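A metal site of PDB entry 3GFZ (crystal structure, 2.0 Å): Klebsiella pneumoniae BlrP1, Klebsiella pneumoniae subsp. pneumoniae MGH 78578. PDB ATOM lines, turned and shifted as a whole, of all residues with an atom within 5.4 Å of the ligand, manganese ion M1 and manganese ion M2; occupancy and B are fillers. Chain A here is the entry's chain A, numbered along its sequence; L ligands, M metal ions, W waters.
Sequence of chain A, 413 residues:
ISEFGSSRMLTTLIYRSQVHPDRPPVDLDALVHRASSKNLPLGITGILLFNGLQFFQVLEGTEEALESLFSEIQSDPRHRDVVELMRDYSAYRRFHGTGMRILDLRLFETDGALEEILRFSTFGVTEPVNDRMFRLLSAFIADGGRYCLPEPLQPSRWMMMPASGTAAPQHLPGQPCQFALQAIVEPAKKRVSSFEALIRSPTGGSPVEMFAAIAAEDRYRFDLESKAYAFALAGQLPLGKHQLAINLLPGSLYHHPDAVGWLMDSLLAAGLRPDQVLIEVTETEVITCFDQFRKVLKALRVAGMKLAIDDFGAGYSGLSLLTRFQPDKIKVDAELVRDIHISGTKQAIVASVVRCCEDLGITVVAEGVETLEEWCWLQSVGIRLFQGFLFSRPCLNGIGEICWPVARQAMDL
N8 of the ligand sits at hydrogen-bond distance from O of Asn 247 (3.4 Å). The side-chain carboxylate of Glu 370 lies within hydrogen-bond range of a nitrogen (N3) of the ligand (2.7 Å). A nitrogen (N8) of the ligand is in hydrogen-bond range of the side-chain carboxylate (OD1) of Asp 223 (2.7 Å). An oxygen (O7) of the ligand sits at hydrogen-bond distance from the backbone NH of Phe 389. NZ of Lys 227 lies within hydrogen-bond range of O14 of the ligand, at 2.9 Å. NH1 of Arg 200 lies within salt-bridge range of O9 of the ligand (3.0 Å). A nitrogen (N2) of the ligand is in hydrogen-bond range of the side-chain amide nitrogen (NE2) of Gln 182 (3.2 Å). The backbone NH (N) of Ile 199 is in hydrogen-bond range of a nitrogen (N7) of the ligand (3.1 Å).
The side-chain amino group (NZ) of Lys 331 is in salt-bridge range of the side-chain carboxylate (OE1) of Glu 280, 2.4 Å away. N of Asp 311 sits at hydrogen-bond distance from O of Lys 331. O of Asn 247 lies close to NZ of Lys 227 (3.2 Å). The side-chain amide nitrogen of Asn 247 lies within hydrogen-bond range of the backbone carbonyl oxygen of Ala 197, at 3.4 Å. The side-chain carboxylate (OD1) of Asp 223 lies within salt-bridge range of the side-chain amino group (NZ) of Lys 227. The side-chain carboxylate (OD2) of Asp 223 sits at hydrogen-bond distance from the backbone NH (N) of Leu 249 (2.9 Å). NZ of Lys 227 lies within hydrogen-bond range of OG of Ser 226, at 3.2 Å. The side-chain amide oxygen of Gln 182 is in hydrogen-bond range of the side-chain amide nitrogen of Gln 387, at 3.0 Å.
Residues that only touch the ligand: Gly 388, Pro 394, Gly 368, Leu 198, Leu 249, Pro 207, Val 369, Phe 211 and Phe 179. Of the 30 residues printed, 21 come within 4 Å of the ligand.
Three residues have an atom within 4 Å of manganese ion M1: Asp 310, Asp 311 and Glu 367. The nearest printed residue that does not touch manganese ion M1 is Glu 280 (5.2 Å).
Four residues have an atom within 4 Å of manganese ion M2: Glu 196, Asn 247, Glu 280 and Asp 310. Along chain A the residues within 4 Å of manganese ion M2 span positions 196 to 310.
Manganese ion M1 is bound by O2 of the ligand, OD1 of Asp 311, OE1 of Glu 367, OD1 of Asp 310 and OE2 of Glu 367. Manganese ion M1 has five donor atoms within binding distance.
Manganese ion M2 is bound by the side-chain carboxylate (OE2) of Glu 280 (1.9 Å). Manganese ion M2 is bound by O1 of the ligand. Manganese ion M2 is bound by OD2 of Asp 310. Manganese ion M2 is bound by OD1 of Asn 247, 2.2 Å away. Manganese ion M2 is bound by OE2 of Glu 196, at 2.2 Å. Water W3 is bound to manganese ion M2, at 2.3 Å. Manganese ion M2 has six donor atoms within binding distance.
Water W3 lies within hydrogen-bond range of OE1 of Glu 196 (3.0 Å), NZ of Lys 331 (3.4 Å) and O3 of the ligand (3.4 Å). Water W4 bridges O13 of the ligand (2.6 Å) and OD2 of Asp 311 (3.2 Å). Water W2 lies within hydrogen-bond range of N of Gly 368 (2.8 Å), N2 of the ligand (3.1 Å) and O of Gln 387 (3.2 Å). Water W5 lies within hydrogen-bond range of the backbone carbonyl oxygen of Ala 197 (2.6 Å), the backbone NH of Asn 247 (3.0 Å) and an oxygen (O14) of the ligand (3.1 Å).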
ATOM      1  N   PHE A 179     -17.015  -0.657 -21.120  1.00  0.00           N
ATOM      2  CA  PHE A 179     -17.327  -1.495 -22.267  1.00  0.00           C
ATOM      3  C   PHE A 179     -16.178  -1.467 -23.234  1.00  0.00           C
ATOM      4  O   PHE A 179     -15.613  -0.407 -23.534  1.00  0.00           O
ATOM      5  CB  PHE A 179     -18.609  -1.038 -22.964  1.00  0.00           C
ATOM      6  CG  PHE A 179     -19.848  -1.408 -22.223  1.00  0.00           C
ATOM      7  CD1 PHE A 179     -20.366  -0.564 -21.265  1.00  0.00           C
ATOM      8  CD2 PHE A 179     -20.466  -2.624 -22.452  1.00  0.00           C
ATOM      9  CE1 PHE A 179     -21.488  -0.911 -20.559  1.00  0.00           C
ATOM     10  CE2 PHE A 179     -21.604  -2.980 -21.761  1.00  0.00           C
ATOM     11  CZ  PHE A 179     -22.120  -2.127 -20.805  1.00  0.00           C
ATOM     12  N   GLN A 182     -15.705  -4.321 -30.060  1.00  0.00           N
ATOM     13  CA  GLN A 182     -15.107  -5.132 -31.114  1.00  0.00           C
ATOM     14  C   GLN A 182     -15.904  -4.917 -32.407  1.00  0.00           C
ATOM     15  O   GLN A 182     -17.138  -4.979 -32.406  1.00  0.00           O
ATOM     16  CB  GLN A 182     -15.099  -6.617 -30.749  1.00  0.00           C
ATOM     17  CG  GLN A 182     -14.429  -7.523 -31.795  1.00  0.00           C
ATOM     18  CD  GLN A 182     -14.313  -8.975 -31.338  1.00  0.00           C
ATOM     19  OE1 GLN A 182     -15.179  -9.498 -30.641  1.00  0.00           O
ATOM     20  NE2 GLN A 182     -13.232  -9.627 -31.741  1.00  0.00           N
ATOM     21  N   GLU A 196     -19.701  -4.396 -31.440  1.00  0.00           N
ATOM     22  CA  GLU A 196     -20.324  -5.037 -30.285  1.00  0.00           C
ATOM     23  C   GLU A 196     -19.731  -4.492 -28.990  1.00  0.00           C
ATOM     24  O   GLU A 196     -18.524  -4.455 -28.842  1.00  0.00           O
ATOM     25  CB  GLU A 196     -20.161  -6.554 -30.302  1.00  0.00           C
ATOM     26  CG  GLU A 196     -20.763  -7.200 -29.071  1.00  0.00           C
ATOM     27  CD  GLU A 196     -20.837  -8.705 -29.122  1.00  0.00           C
ATOM     28  OE1 GLU A 196     -20.243  -9.320 -30.033  1.00  0.00           O
ATOM     29  OE2 GLU A 196     -21.540  -9.254 -28.231  1.00  0.00           O
ATOM     30  N   ALA A 197     -20.611  -4.115 -28.057  1.00  0.00           N
ATOM     31  CA  ALA A 197     -20.215  -3.640 -26.740  1.00  0.00           C
ATOM     32  C   ALA A 197     -20.094  -4.825 -25.765  1.00  0.00           C
ATOM     33  O   ALA A 197     -21.055  -5.535 -25.508  1.00  0.00           O
ATOM     34  CB  ALA A 197     -21.230  -2.647 -26.230  1.00  0.00           C
ATOM     35  N   LEU A 198     -18.897  -4.997 -25.210  1.00  0.00           N
ATOM     36  CA  LEU A 198     -18.583  -6.096 -24.296  1.00  0.00           C
ATOM     37  C   LEU A 198     -18.255  -5.527 -22.918  1.00  0.00           C
ATOM     38  O   LEU A 198     -17.300  -4.782 -22.777  1.00  0.00           O
ATOM     39  CB  LEU A 198     -17.393  -6.881 -24.835  1.00  0.00           C
ATOM     40  CG  LEU A 198     -17.529  -7.373 -26.273  1.00  0.00           C
ATOM     41  CD1 LEU A 198     -16.203  -7.916 -26.798  1.00  0.00           C
ATOM     42  CD2 LEU A 198     -18.661  -8.407 -26.379  1.00  0.00           C
ATOM     43  N   ILE A 199     -19.043  -5.898 -21.902  1.00  0.00           N
ATOM     44  CA  ILE A 199     -18.926  -5.245 -20.596  1.00  0.00           C
ATOM     45  C   ILE A 199     -17.631  -5.613 -19.902  1.00  0.00           C
ATOM     46  O   ILE A 199     -17.142  -6.745 -20.013  1.00  0.00           O
ATOM     47  CB  ILE A 199     -20.129  -5.567 -19.674  1.00  0.00           C
ATOM     48  CG1 ILE A 199     -20.229  -4.534 -18.530  1.00  0.00           C
ATOM     49  CG2 ILE A 199     -20.042  -7.000 -19.122  1.00  0.00           C
ATOM     50  CD1 ILE A 199     -21.583  -4.539 -17.841  1.00  0.00           C
ATOM     51  N   ARG A 200     -17.078  -4.645 -19.181  1.00  0.00           N
ATOM     52  CA  ARG A 200     -15.838  -4.801 -18.447  1.00  0.00           C
ATOM     53  C   ARG A 200     -15.996  -4.217 -17.063  1.00  0.00           C
ATOM     54  O   ARG A 200     -16.864  -3.374 -16.834  1.00  0.00           O
ATOM     55  CB  ARG A 200     -14.717  -4.077 -19.183  1.00  0.00           C
ATOM     56  CG  ARG A 200     -14.425  -4.614 -20.555  1.00  0.00           C
ATOM     57  CD  ARG A 200     -13.600  -5.867 -20.468  1.00  0.00           C
ATOM     58  NE  ARG A 200     -13.342  -6.451 -21.778  1.00  0.00           N
ATOM     59  CZ  ARG A 200     -14.116  -7.340 -22.398  1.00  0.00           C
ATOM     60  NH1 ARG A 200     -15.214  -7.804 -21.832  1.00  0.00           N
ATOM     61  NH2 ARG A 200     -13.756  -7.784 -23.597  1.00  0.00           N
ATOM     62  N   SER A 206     -12.926  -8.993 -16.891  1.00  0.00           N
ATOM     63  CA  SER A 206     -13.900  -9.690 -17.747  1.00  0.00           C
ATOM     64  C   SER A 206     -15.350  -9.490 -17.274  1.00  0.00           C
ATOM     65  O   SER A 206     -15.558  -9.044 -16.145  1.00  0.00           O
ATOM     66  CB  SER A 206     -13.588 -11.193 -17.749  1.00  0.00           C
ATOM     67  OG  SER A 206     -13.842 -11.744 -16.451  1.00  0.00           O
ATOM     68  N   PRO A 207     -16.340  -9.822 -18.128  1.00  0.00           N
ATOM     69  CA  PRO A 207     -17.758  -9.783 -17.729  1.00  0.00           C
ATOM     70  C   PRO A 207     -18.060 -10.620 -16.486  1.00  0.00           C
ATOM     71  O   PRO A 207     -18.853 -10.200 -15.637  1.00  0.00           O
ATOM     72  CB  PRO A 207     -18.487 -10.363 -18.950  1.00  0.00           C
ATOM     73  CG  PRO A 207     -17.603 -10.058 -20.078  1.00  0.00           C
ATOM     74  CD  PRO A 207     -16.212 -10.240 -19.540  1.00  0.00           C
ATOM     75  N   PHE A 211     -19.744  -9.127 -13.194  1.00  0.00           N
ATOM     76  CA  PHE A 211     -20.987  -9.618 -12.583  1.00  0.00           C
ATOM     77  C   PHE A 211     -20.812 -10.297 -11.223  1.00  0.00           C
ATOM     78  O   PHE A 211     -21.742 -10.309 -10.423  1.00  0.00           O
ATOM     79  CB  PHE A 211     -21.757 -10.523 -13.540  1.00  0.00           C
ATOM     80  CG  PHE A 211     -22.528  -9.773 -14.576  1.00  0.00           C
ATOM     81  CD1 PHE A 211     -23.688  -9.093 -14.234  1.00  0.00           C
ATOM     82  CD2 PHE A 211     -22.104  -9.731 -15.891  1.00  0.00           C
ATOM     83  CE1 PHE A 211     -24.410  -8.390 -15.174  1.00  0.00           C
ATOM     84  CE2 PHE A 211     -22.822  -9.030 -16.839  1.00  0.00           C
ATOM     85  CZ  PHE A 211     -23.979  -8.359 -16.483  1.00  0.00           C
ATOM     86  N   ASP A 223     -27.358  -5.546 -15.375  1.00  0.00           N
ATOM     87  CA  ASP A 223     -27.110  -5.872 -16.780  1.00  0.00           C
ATOM     88  C   ASP A 223     -27.808  -4.882 -17.685  1.00  0.00           C
ATOM     89  O   ASP A 223     -27.222  -4.371 -18.649  1.00  0.00           O
ATOM     90  CB  ASP A 223     -27.618  -7.294 -17.072  1.00  0.00           C
ATOM     91  CG  ASP A 223     -27.335  -7.733 -18.493  1.00  0.00           C
ATOM     92  OD1 ASP A 223     -26.350  -7.259 -19.074  1.00  0.00           O
ATOM     93  OD2 ASP A 223     -28.111  -8.560 -19.039  1.00  0.00           O
ATOM     94  N   SER A 226     -26.557  -1.064 -17.008  1.00  0.00           N
ATOM     95  CA  SER A 226     -25.217  -0.858 -17.527  1.00  0.00           C
ATOM     96  C   SER A 226     -25.205  -0.361 -18.968  1.00  0.00           C
ATOM     97  O   SER A 226     -24.248   0.253 -19.394  1.00  0.00           O
ATOM     98  CB  SER A 226     -24.382  -2.146 -17.450  1.00  0.00           C
ATOM     99  OG  SER A 226     -24.856  -3.134 -18.354  1.00  0.00           O
ATOM    100  N   LYS A 227     -26.281  -0.630 -19.707  1.00  0.00           N
ATOM    101  CA  LYS A 227     -26.353  -0.278 -21.128  1.00  0.00           C
ATOM    102  C   LYS A 227     -26.345   1.223 -21.424  1.00  0.00           C
ATOM    103  O   LYS A 227     -25.951   1.631 -22.511  1.00  0.00           O
ATOM    104  CB  LYS A 227     -27.548  -0.986 -21.785  1.00  0.00           C
ATOM    105  CG  LYS A 227     -27.481  -2.523 -21.716  1.00  0.00           C
ATOM    106  CD  LYS A 227     -26.087  -3.037 -22.087  1.00  0.00           C
ATOM    107  CE  LYS A 227     -25.998  -4.529 -22.029  1.00  0.00           C
ATOM    108  NZ  LYS A 227     -25.749  -5.090 -20.676  1.00  0.00           N
ATOM    109  N   ASN A 247     -25.352  -6.963 -25.585  1.00  0.00           N
ATOM    110  CA  ASN A 247     -25.715  -8.253 -25.019  1.00  0.00           C
ATOM    111  C   ASN A 247     -26.602  -8.062 -23.804  1.00  0.00           C
ATOM    112  O   ASN A 247     -26.274  -7.264 -22.929  1.00  0.00           O
ATOM    113  CB  ASN A 247     -24.480  -9.022 -24.560  1.00  0.00           C
ATOM    114  CG  ASN A 247     -23.574  -9.381 -25.696  1.00  0.00           C
ATOM    115  OD1 ASN A 247     -23.855 -10.314 -26.446  1.00  0.00           O
ATOM    116  ND2 ASN A 247     -22.459  -8.664 -25.825  1.00  0.00           N
ATOM    117  N   LEU A 248     -27.705  -8.799 -23.732  1.00  0.00           N
ATOM    118  CA  LEU A 248     -28.599  -8.737 -22.569  1.00  0.00           C
ATOM    119  C   LEU A 248     -29.160 -10.115 -22.253  1.00  0.00           C
ATOM    120  O   LEU A 248     -29.447 -10.884 -23.162  1.00  0.00           O
ATOM    121  CB  LEU A 248     -29.765  -7.771 -22.845  1.00  0.00           C
ATOM    122  CG  LEU A 248     -29.586  -6.275 -22.561  1.00  0.00           C
ATOM    123  CD1 LEU A 248     -30.831  -5.493 -23.016  1.00  0.00           C
ATOM    124  CD2 LEU A 248     -29.329  -5.999 -21.091  1.00  0.00           C
ATOM    125  N   LEU A 249     -29.299 -10.412 -20.963  1.00  0.00           N
ATOM    126  CA  LEU A 249     -30.013 -11.607 -20.519  1.00  0.00           C
ATOM    127  C   LEU A 249     -31.496 -11.365 -20.754  1.00  0.00           C
ATOM    128  O   LEU A 249     -32.010 -10.292 -20.431  1.00  0.00           O
ATOM    129  CB  LEU A 249     -29.785 -11.857 -19.022  1.00  0.00           C
ATOM    130  CG  LEU A 249     -28.359 -12.082 -18.527  1.00  0.00           C
ATOM    131  CD1 LEU A 249     -28.303 -11.996 -17.011  1.00  0.00           C
ATOM    132  CD2 LEU A 249     -27.814 -13.410 -19.002  1.00  0.00           C
ATOM    133  N   GLU A 280     -28.419  -8.495 -28.567  1.00  0.00           N
ATOM    134  CA  GLU A 280     -27.970  -9.885 -28.670  1.00  0.00           C
ATOM    135  C   GLU A 280     -28.467 -10.701 -27.480  1.00  0.00           C
ATOM    136  O   GLU A 280     -28.156 -10.379 -26.341  1.00  0.00           O
ATOM    137  CB  GLU A 280     -26.449  -9.990 -28.726  1.00  0.00           C
ATOM    138  CG  GLU A 280     -25.831  -9.235 -29.885  1.00  0.00           C
ATOM    139  CD  GLU A 280     -24.423  -9.689 -30.242  1.00  0.00           C
ATOM    140  OE1 GLU A 280     -23.894  -9.195 -31.259  1.00  0.00           O
ATOM    141  OE2 GLU A 280     -23.827 -10.508 -29.505  1.00  0.00           O
ATOM    142  N   THR A 282     -28.592 -14.880 -26.331  1.00  0.00           N
ATOM    143  CA  THR A 282     -28.053 -16.179 -26.682  1.00  0.00           C
ATOM    144  C   THR A 282     -29.188 -17.176 -26.820  1.00  0.00           C
ATOM    145  O   THR A 282     -30.144 -17.156 -26.049  1.00  0.00           O
ATOM    146  CB  THR A 282     -27.054 -16.729 -25.651  1.00  0.00           C
ATOM    147  OG1 THR A 282     -27.657 -16.707 -24.359  1.00  0.00           O
ATOM    148  CG2 THR A 282     -25.797 -15.908 -25.645  1.00  0.00           C
ATOM    149  N   ASP A 310     -27.288 -14.777 -30.608  1.00  0.00           N
ATOM    150  CA  ASP A 310     -25.859 -14.898 -30.388  1.00  0.00           C
ATOM    151  C   ASP A 310     -25.553 -16.376 -30.145  1.00  0.00           C
ATOM    152  O   ASP A 310     -26.420 -17.117 -29.687  1.00  0.00           O
ATOM    153  CB  ASP A 310     -25.513 -14.074 -29.147  1.00  0.00           C
ATOM    154  CG  ASP A 310     -24.060 -13.673 -29.066  1.00  0.00           C
ATOM    155  OD1 ASP A 310     -23.247 -13.954 -29.994  1.00  0.00           O
ATOM    156  OD2 ASP A 310     -23.724 -13.002 -28.049  1.00  0.00           O
ATOM    157  N   ASP A 311     -24.331 -16.788 -30.466  1.00  0.00           N
ATOM    158  CA  ASP A 311     -23.879 -18.172 -30.226  1.00  0.00           C
ATOM    159  C   ASP A 311     -24.829 -19.196 -30.812  1.00  0.00           C
ATOM    160  O   ASP A 311     -25.106 -20.231 -30.211  1.00  0.00           O
ATOM    161  CB  ASP A 311     -23.676 -18.436 -28.726  1.00  0.00           C
ATOM    162  CG  ASP A 311     -22.723 -17.457 -28.085  1.00  0.00           C
ATOM    163  OD1 ASP A 311     -21.847 -16.928 -28.802  1.00  0.00           O
ATOM    164  OD2 ASP A 311     -22.844 -17.233 -26.871  1.00  0.00           O
ATOM    165  N   LYS A 331     -25.697 -14.989 -35.182  1.00  0.00           N
ATOM    166  CA  LYS A 331     -24.244 -15.022 -35.039  1.00  0.00           C
ATOM    167  C   LYS A 331     -23.839 -16.475 -34.837  1.00  0.00           C
ATOM    168  O   LYS A 331     -24.189 -17.068 -33.834  1.00  0.00           O
ATOM    169  CB  LYS A 331     -23.807 -14.136 -33.884  1.00  0.00           C
ATOM    170  CG  LYS A 331     -24.373 -12.731 -33.987  1.00  0.00           C
ATOM    171  CD  LYS A 331     -23.812 -11.799 -32.923  1.00  0.00           C
ATOM    172  CE  LYS A 331     -22.470 -11.250 -33.341  1.00  0.00           C
ATOM    173  NZ  LYS A 331     -22.063 -10.069 -32.551  1.00  0.00           N
ATOM    174  N   GLU A 367     -18.609 -15.785 -35.701  1.00  0.00           N
ATOM    175  CA  GLU A 367     -17.864 -15.389 -34.521  1.00  0.00           C
ATOM    176  C   GLU A 367     -16.608 -16.216 -34.305  1.00  0.00           C
ATOM    177  O   GLU A 367     -16.552 -17.365 -34.713  1.00  0.00           O
ATOM    178  CB  GLU A 367     -18.678 -15.606 -33.252  1.00  0.00           C
ATOM    179  CG  GLU A 367     -20.005 -14.969 -33.168  1.00  0.00           C
ATOM    180  CD  GLU A 367     -20.534 -15.037 -31.748  1.00  0.00           C
ATOM    181  OE1 GLU A 367     -19.997 -14.305 -30.893  1.00  0.00           O
ATOM    182  OE2 GLU A 367     -21.462 -15.832 -31.469  1.00  0.00           O
ATOM    183  N   GLY A 368     -15.656 -15.637 -33.587  1.00  0.00           N
ATOM    184  CA  GLY A 368     -14.465 -16.369 -33.143  1.00  0.00           C
ATOM    185  C   GLY A 368     -13.485 -16.688 -34.258  1.00  0.00           C
ATOM    186  O   GLY A 368     -12.765 -17.674 -34.174  1.00  0.00           O
ATOM    187  N   VAL A 369     -13.447 -15.828 -35.272  1.00  0.00           N
ATOM    188  CA  VAL A 369     -12.602 -16.058 -36.452  1.00  0.00           C
ATOM    189  C   VAL A 369     -11.156 -15.632 -36.126  1.00  0.00           C
ATOM    190  O   VAL A 369     -10.868 -14.444 -35.982  1.00  0.00           O
ATOM    191  CB  VAL A 369     -13.148 -15.298 -37.696  1.00  0.00           C
ATOM    192  CG1 VAL A 369     -12.374 -15.677 -38.937  1.00  0.00           C
ATOM    193  CG2 VAL A 369     -14.611 -15.626 -37.929  1.00  0.00           C
ATOM    194  N   GLU A 370     -10.278 -16.612 -35.999  1.00  0.00           N
ATOM    195  CA  GLU A 370      -8.923 -16.424 -35.514  1.00  0.00           C
ATOM    196  C   GLU A 370      -7.837 -16.571 -36.568  1.00  0.00           C
ATOM    197  O   GLU A 370      -6.736 -16.064 -36.380  1.00  0.00           O
ATOM    198  CB  GLU A 370      -8.659 -17.420 -34.379  1.00  0.00           C
ATOM    199  CG  GLU A 370      -9.573 -17.218 -33.200  1.00  0.00           C
ATOM    200  CD  GLU A 370      -9.220 -18.057 -31.995  1.00  0.00           C
ATOM    201  OE1 GLU A 370      -8.542 -19.107 -32.135  1.00  0.00           O
ATOM    202  OE2 GLU A 370      -9.643 -17.676 -30.896  1.00  0.00           O
ATOM    203  N   GLN A 387     -16.530 -11.609 -37.103  1.00  0.00           N
ATOM    204  CA  GLN A 387     -16.123 -11.050 -35.833  1.00  0.00           C
ATOM    205  C   GLN A 387     -15.065 -11.987 -35.278  1.00  0.00           C
ATOM    206  O   GLN A 387     -15.285 -13.178 -35.127  1.00  0.00           O
ATOM    207  CB  GLN A 387     -17.320 -10.970 -34.899  1.00  0.00           C
ATOM    208  CG  GLN A 387     -17.046 -10.140 -33.644  1.00  0.00           C
ATOM    209  CD  GLN A 387     -18.224 -10.077 -32.731  1.00  0.00           C
ATOM    210  OE1 GLN A 387     -19.343 -10.452 -33.110  1.00  0.00           O
ATOM    211  NE2 GLN A 387     -18.006  -9.601 -31.509  1.00  0.00           N
ATOM    212  N   GLY A 388     -13.893 -11.440 -34.992  1.00  0.00           N
ATOM    213  CA  GLY A 388     -12.865 -12.242 -34.401  1.00  0.00           C
ATOM    214  C   GLY A 388     -11.560 -11.500 -34.303  1.00  0.00           C
ATOM    215  O   GLY A 388     -11.357 -10.456 -34.935  1.00  0.00           O
ATOM    216  N   PHE A 389     -10.666 -12.084 -33.517  1.00  0.00           N
ATOM    217  CA  PHE A 389      -9.349 -11.532 -33.283  1.00  0.00           C
ATOM    218  C   PHE A 389      -8.506 -11.413 -34.551  1.00  0.00           C
ATOM    219  O   PHE A 389      -7.557 -10.639 -34.585  1.00  0.00           O
ATOM    220  CB  PHE A 389      -8.602 -12.395 -32.276  1.00  0.00           C
ATOM    221  CG  PHE A 389      -9.210 -12.420 -30.887  1.00  0.00           C
ATOM    222  CD1 PHE A 389     -10.117 -11.459 -30.458  1.00  0.00           C
ATOM    223  CD2 PHE A 389      -8.834 -13.412 -30.004  1.00  0.00           C
ATOM    224  CE1 PHE A 389     -10.628 -11.498 -29.170  1.00  0.00           C
ATOM    225  CE2 PHE A 389      -9.354 -13.449 -28.720  1.00  0.00           C
ATOM    226  CZ  PHE A 389     -10.240 -12.495 -28.314  1.00  0.00           C
ATOM    227  N   LEU A 390      -8.831 -12.183 -35.598  1.00  0.00           N
ATOM    228  CA  LEU A 390      -8.148 -12.043 -36.870  1.00  0.00           C
ATOM    229  C   LEU A 390      -8.247 -10.619 -37.425  1.00  0.00           C
ATOM    230  O   LEU A 390      -7.275 -10.084 -37.959  1.00  0.00           O
ATOM    231  CB  LEU A 390      -8.701 -13.033 -37.896  1.00  0.00           C
ATOM    232  CG  LEU A 390      -7.966 -13.089 -39.247  1.00  0.00           C
ATOM    233  CD1 LEU A 390      -6.592 -13.711 -39.083  1.00  0.00           C
ATOM    234  CD2 LEU A 390      -8.784 -13.859 -40.254  1.00  0.00           C
ATOM    235  N   PRO A 394     -11.156  -6.632 -29.128  1.00  0.00           N
ATOM    236  CA  PRO A 394     -11.908  -5.671 -28.326  1.00  0.00           C
ATOM    237  C   PRO A 394     -11.004  -4.586 -27.740  1.00  0.00           C
ATOM    238  O   PRO A 394      -9.872  -4.867 -27.321  1.00  0.00           O
ATOM    239  CB  PRO A 394     -12.497  -6.520 -27.211  1.00  0.00           C
ATOM    240  CG  PRO A 394     -12.575  -7.881 -27.782  1.00  0.00           C
ATOM    241  CD  PRO A 394     -11.381  -8.013 -28.651  1.00  0.00           C
HETATM  242  P1  LIG L   1     -20.238 -12.985 -26.779  1.00  0.00           P
HETATM  243  O1  LIG L   1     -21.193 -11.806 -26.772  1.00  0.00           O
HETATM  244  O2  LIG L   1     -20.729 -14.244 -27.432  1.00  0.00           O
HETATM  245  O3  LIG L   1     -18.922 -12.728 -27.629  1.00  0.00           O
HETATM  246  C1  LIG L   1     -17.851 -11.879 -27.319  1.00  0.00           C
HETATM  247  C2  LIG L   1     -16.705 -12.690 -26.700  1.00  0.00           C
HETATM  248  O4  LIG L   1     -15.906 -13.469 -27.600  1.00  0.00           O
HETATM  249  C3  LIG L   1     -15.743 -11.673 -26.141  1.00  0.00           C
HETATM  250  O5  LIG L   1     -15.256 -12.157 -24.928  1.00  0.00           O
HETATM  251  C4  LIG L   1     -14.609 -11.658 -27.078  1.00  0.00           C
HETATM  252  O6  LIG L   1     -13.548 -10.970 -26.671  1.00  0.00           O
HETATM  253  C5  LIG L   1     -14.572 -12.851 -27.683  1.00  0.00           C
HETATM  254  N1  LIG L   1     -13.958 -13.018 -28.894  1.00  0.00           N
HETATM  255  C6  LIG L   1     -14.211 -12.265 -29.905  1.00  0.00           C
HETATM  256  N2  LIG L   1     -13.506 -12.699 -30.909  1.00  0.00           N
HETATM  257  C7  LIG L   1     -12.794 -13.788 -30.540  1.00  0.00           C
HETATM  258  C8  LIG L   1     -11.893 -14.635 -31.195  1.00  0.00           C
HETATM  259  O7  LIG L   1     -11.592 -14.481 -32.397  1.00  0.00           O
HETATM  260  N3  LIG L   1     -11.359 -15.642 -30.498  1.00  0.00           N
HETATM  261  C9  LIG L   1     -11.665 -15.844 -29.199  1.00  0.00           C
HETATM  262  N4  LIG L   1     -11.069 -16.885 -28.579  1.00  0.00           N
HETATM  263  N5  LIG L   1     -12.525 -15.044 -28.528  1.00  0.00           N
HETATM  264  C10 LIG L   1     -13.097 -14.005 -29.204  1.00  0.00           C
HETATM  265  P2  LIG L   1     -15.813 -11.493 -23.615  1.00  0.00           P
HETATM  266  O8  LIG L   1     -14.723 -11.801 -22.489  1.00  0.00           O
HETATM  267  O9  LIG L   1     -15.814  -9.916 -23.820  1.00  0.00           O
HETATM  268  O10 LIG L   1     -17.371 -11.823 -23.412  1.00  0.00           O
HETATM  269  C11 LIG L   1     -17.754 -13.048 -22.780  1.00  0.00           C
HETATM  270  C12 LIG L   1     -19.274 -13.026 -22.949  1.00  0.00           C
HETATM  271  O11 LIG L   1     -19.885 -12.323 -21.877  1.00  0.00           O
HETATM  272  C13 LIG L   1     -19.900 -12.428 -24.212  1.00  0.00           C
HETATM  273  O12 LIG L   1     -19.860 -13.375 -25.267  1.00  0.00           O
HETATM  274  C14 LIG L   1     -21.272 -12.076 -23.719  1.00  0.00           C
HETATM  275  O13 LIG L   1     -22.003 -13.188 -23.510  1.00  0.00           O
HETATM  276  C15 LIG L   1     -20.890 -11.547 -22.552  1.00  0.00           C
HETATM  277  N6  LIG L   1     -21.248 -10.277 -22.219  1.00  0.00           N
HETATM  278  C16 LIG L   1     -20.461  -9.274 -22.613  1.00  0.00           C
HETATM  279  N7  LIG L   1     -21.096  -8.143 -22.198  1.00  0.00           N
HETATM  280  C17 LIG L   1     -22.248  -8.485 -21.571  1.00  0.00           C
HETATM  281  C18 LIG L   1     -23.247  -7.741 -20.977  1.00  0.00           C
HETATM  282  O14 LIG L   1     -23.173  -6.497 -20.957  1.00  0.00           O
HETATM  283  N8  LIG L   1     -24.309  -8.388 -20.422  1.00  0.00           N
HETATM  284  C19 LIG L   1     -24.390  -9.747 -20.464  1.00  0.00           C
HETATM  285  N9  LIG L   1     -25.449 -10.396 -19.918  1.00  0.00           N
HETATM  286  N10 LIG L   1     -23.428 -10.493 -21.050  1.00  0.00           N
HETATM  287  C20 LIG L   1     -22.358  -9.878 -21.606  1.00  0.00           C
HETATM  288 MN    MN M   1     -21.229 -14.961 -29.236  1.00  0.00          MN
HETATM  289 MN    MN M   2     -22.670 -11.174 -28.118  1.00  0.00          MN
HETATM  290  O   HOH W   1     -12.196 -12.040 -24.805  1.00  0.00           O
HETATM  291  O   HOH W   2     -16.263 -13.352 -32.080  1.00  0.00           O
HETATM  292  O   HOH W   3     -21.416 -12.038 -29.872  1.00  0.00           O
HETATM  293  O   HOH W   4     -23.054 -14.278 -25.679  1.00  0.00           O
HETATM  294  O   HOH W   5     -23.151  -5.701 -23.940  1.00  0.00           O
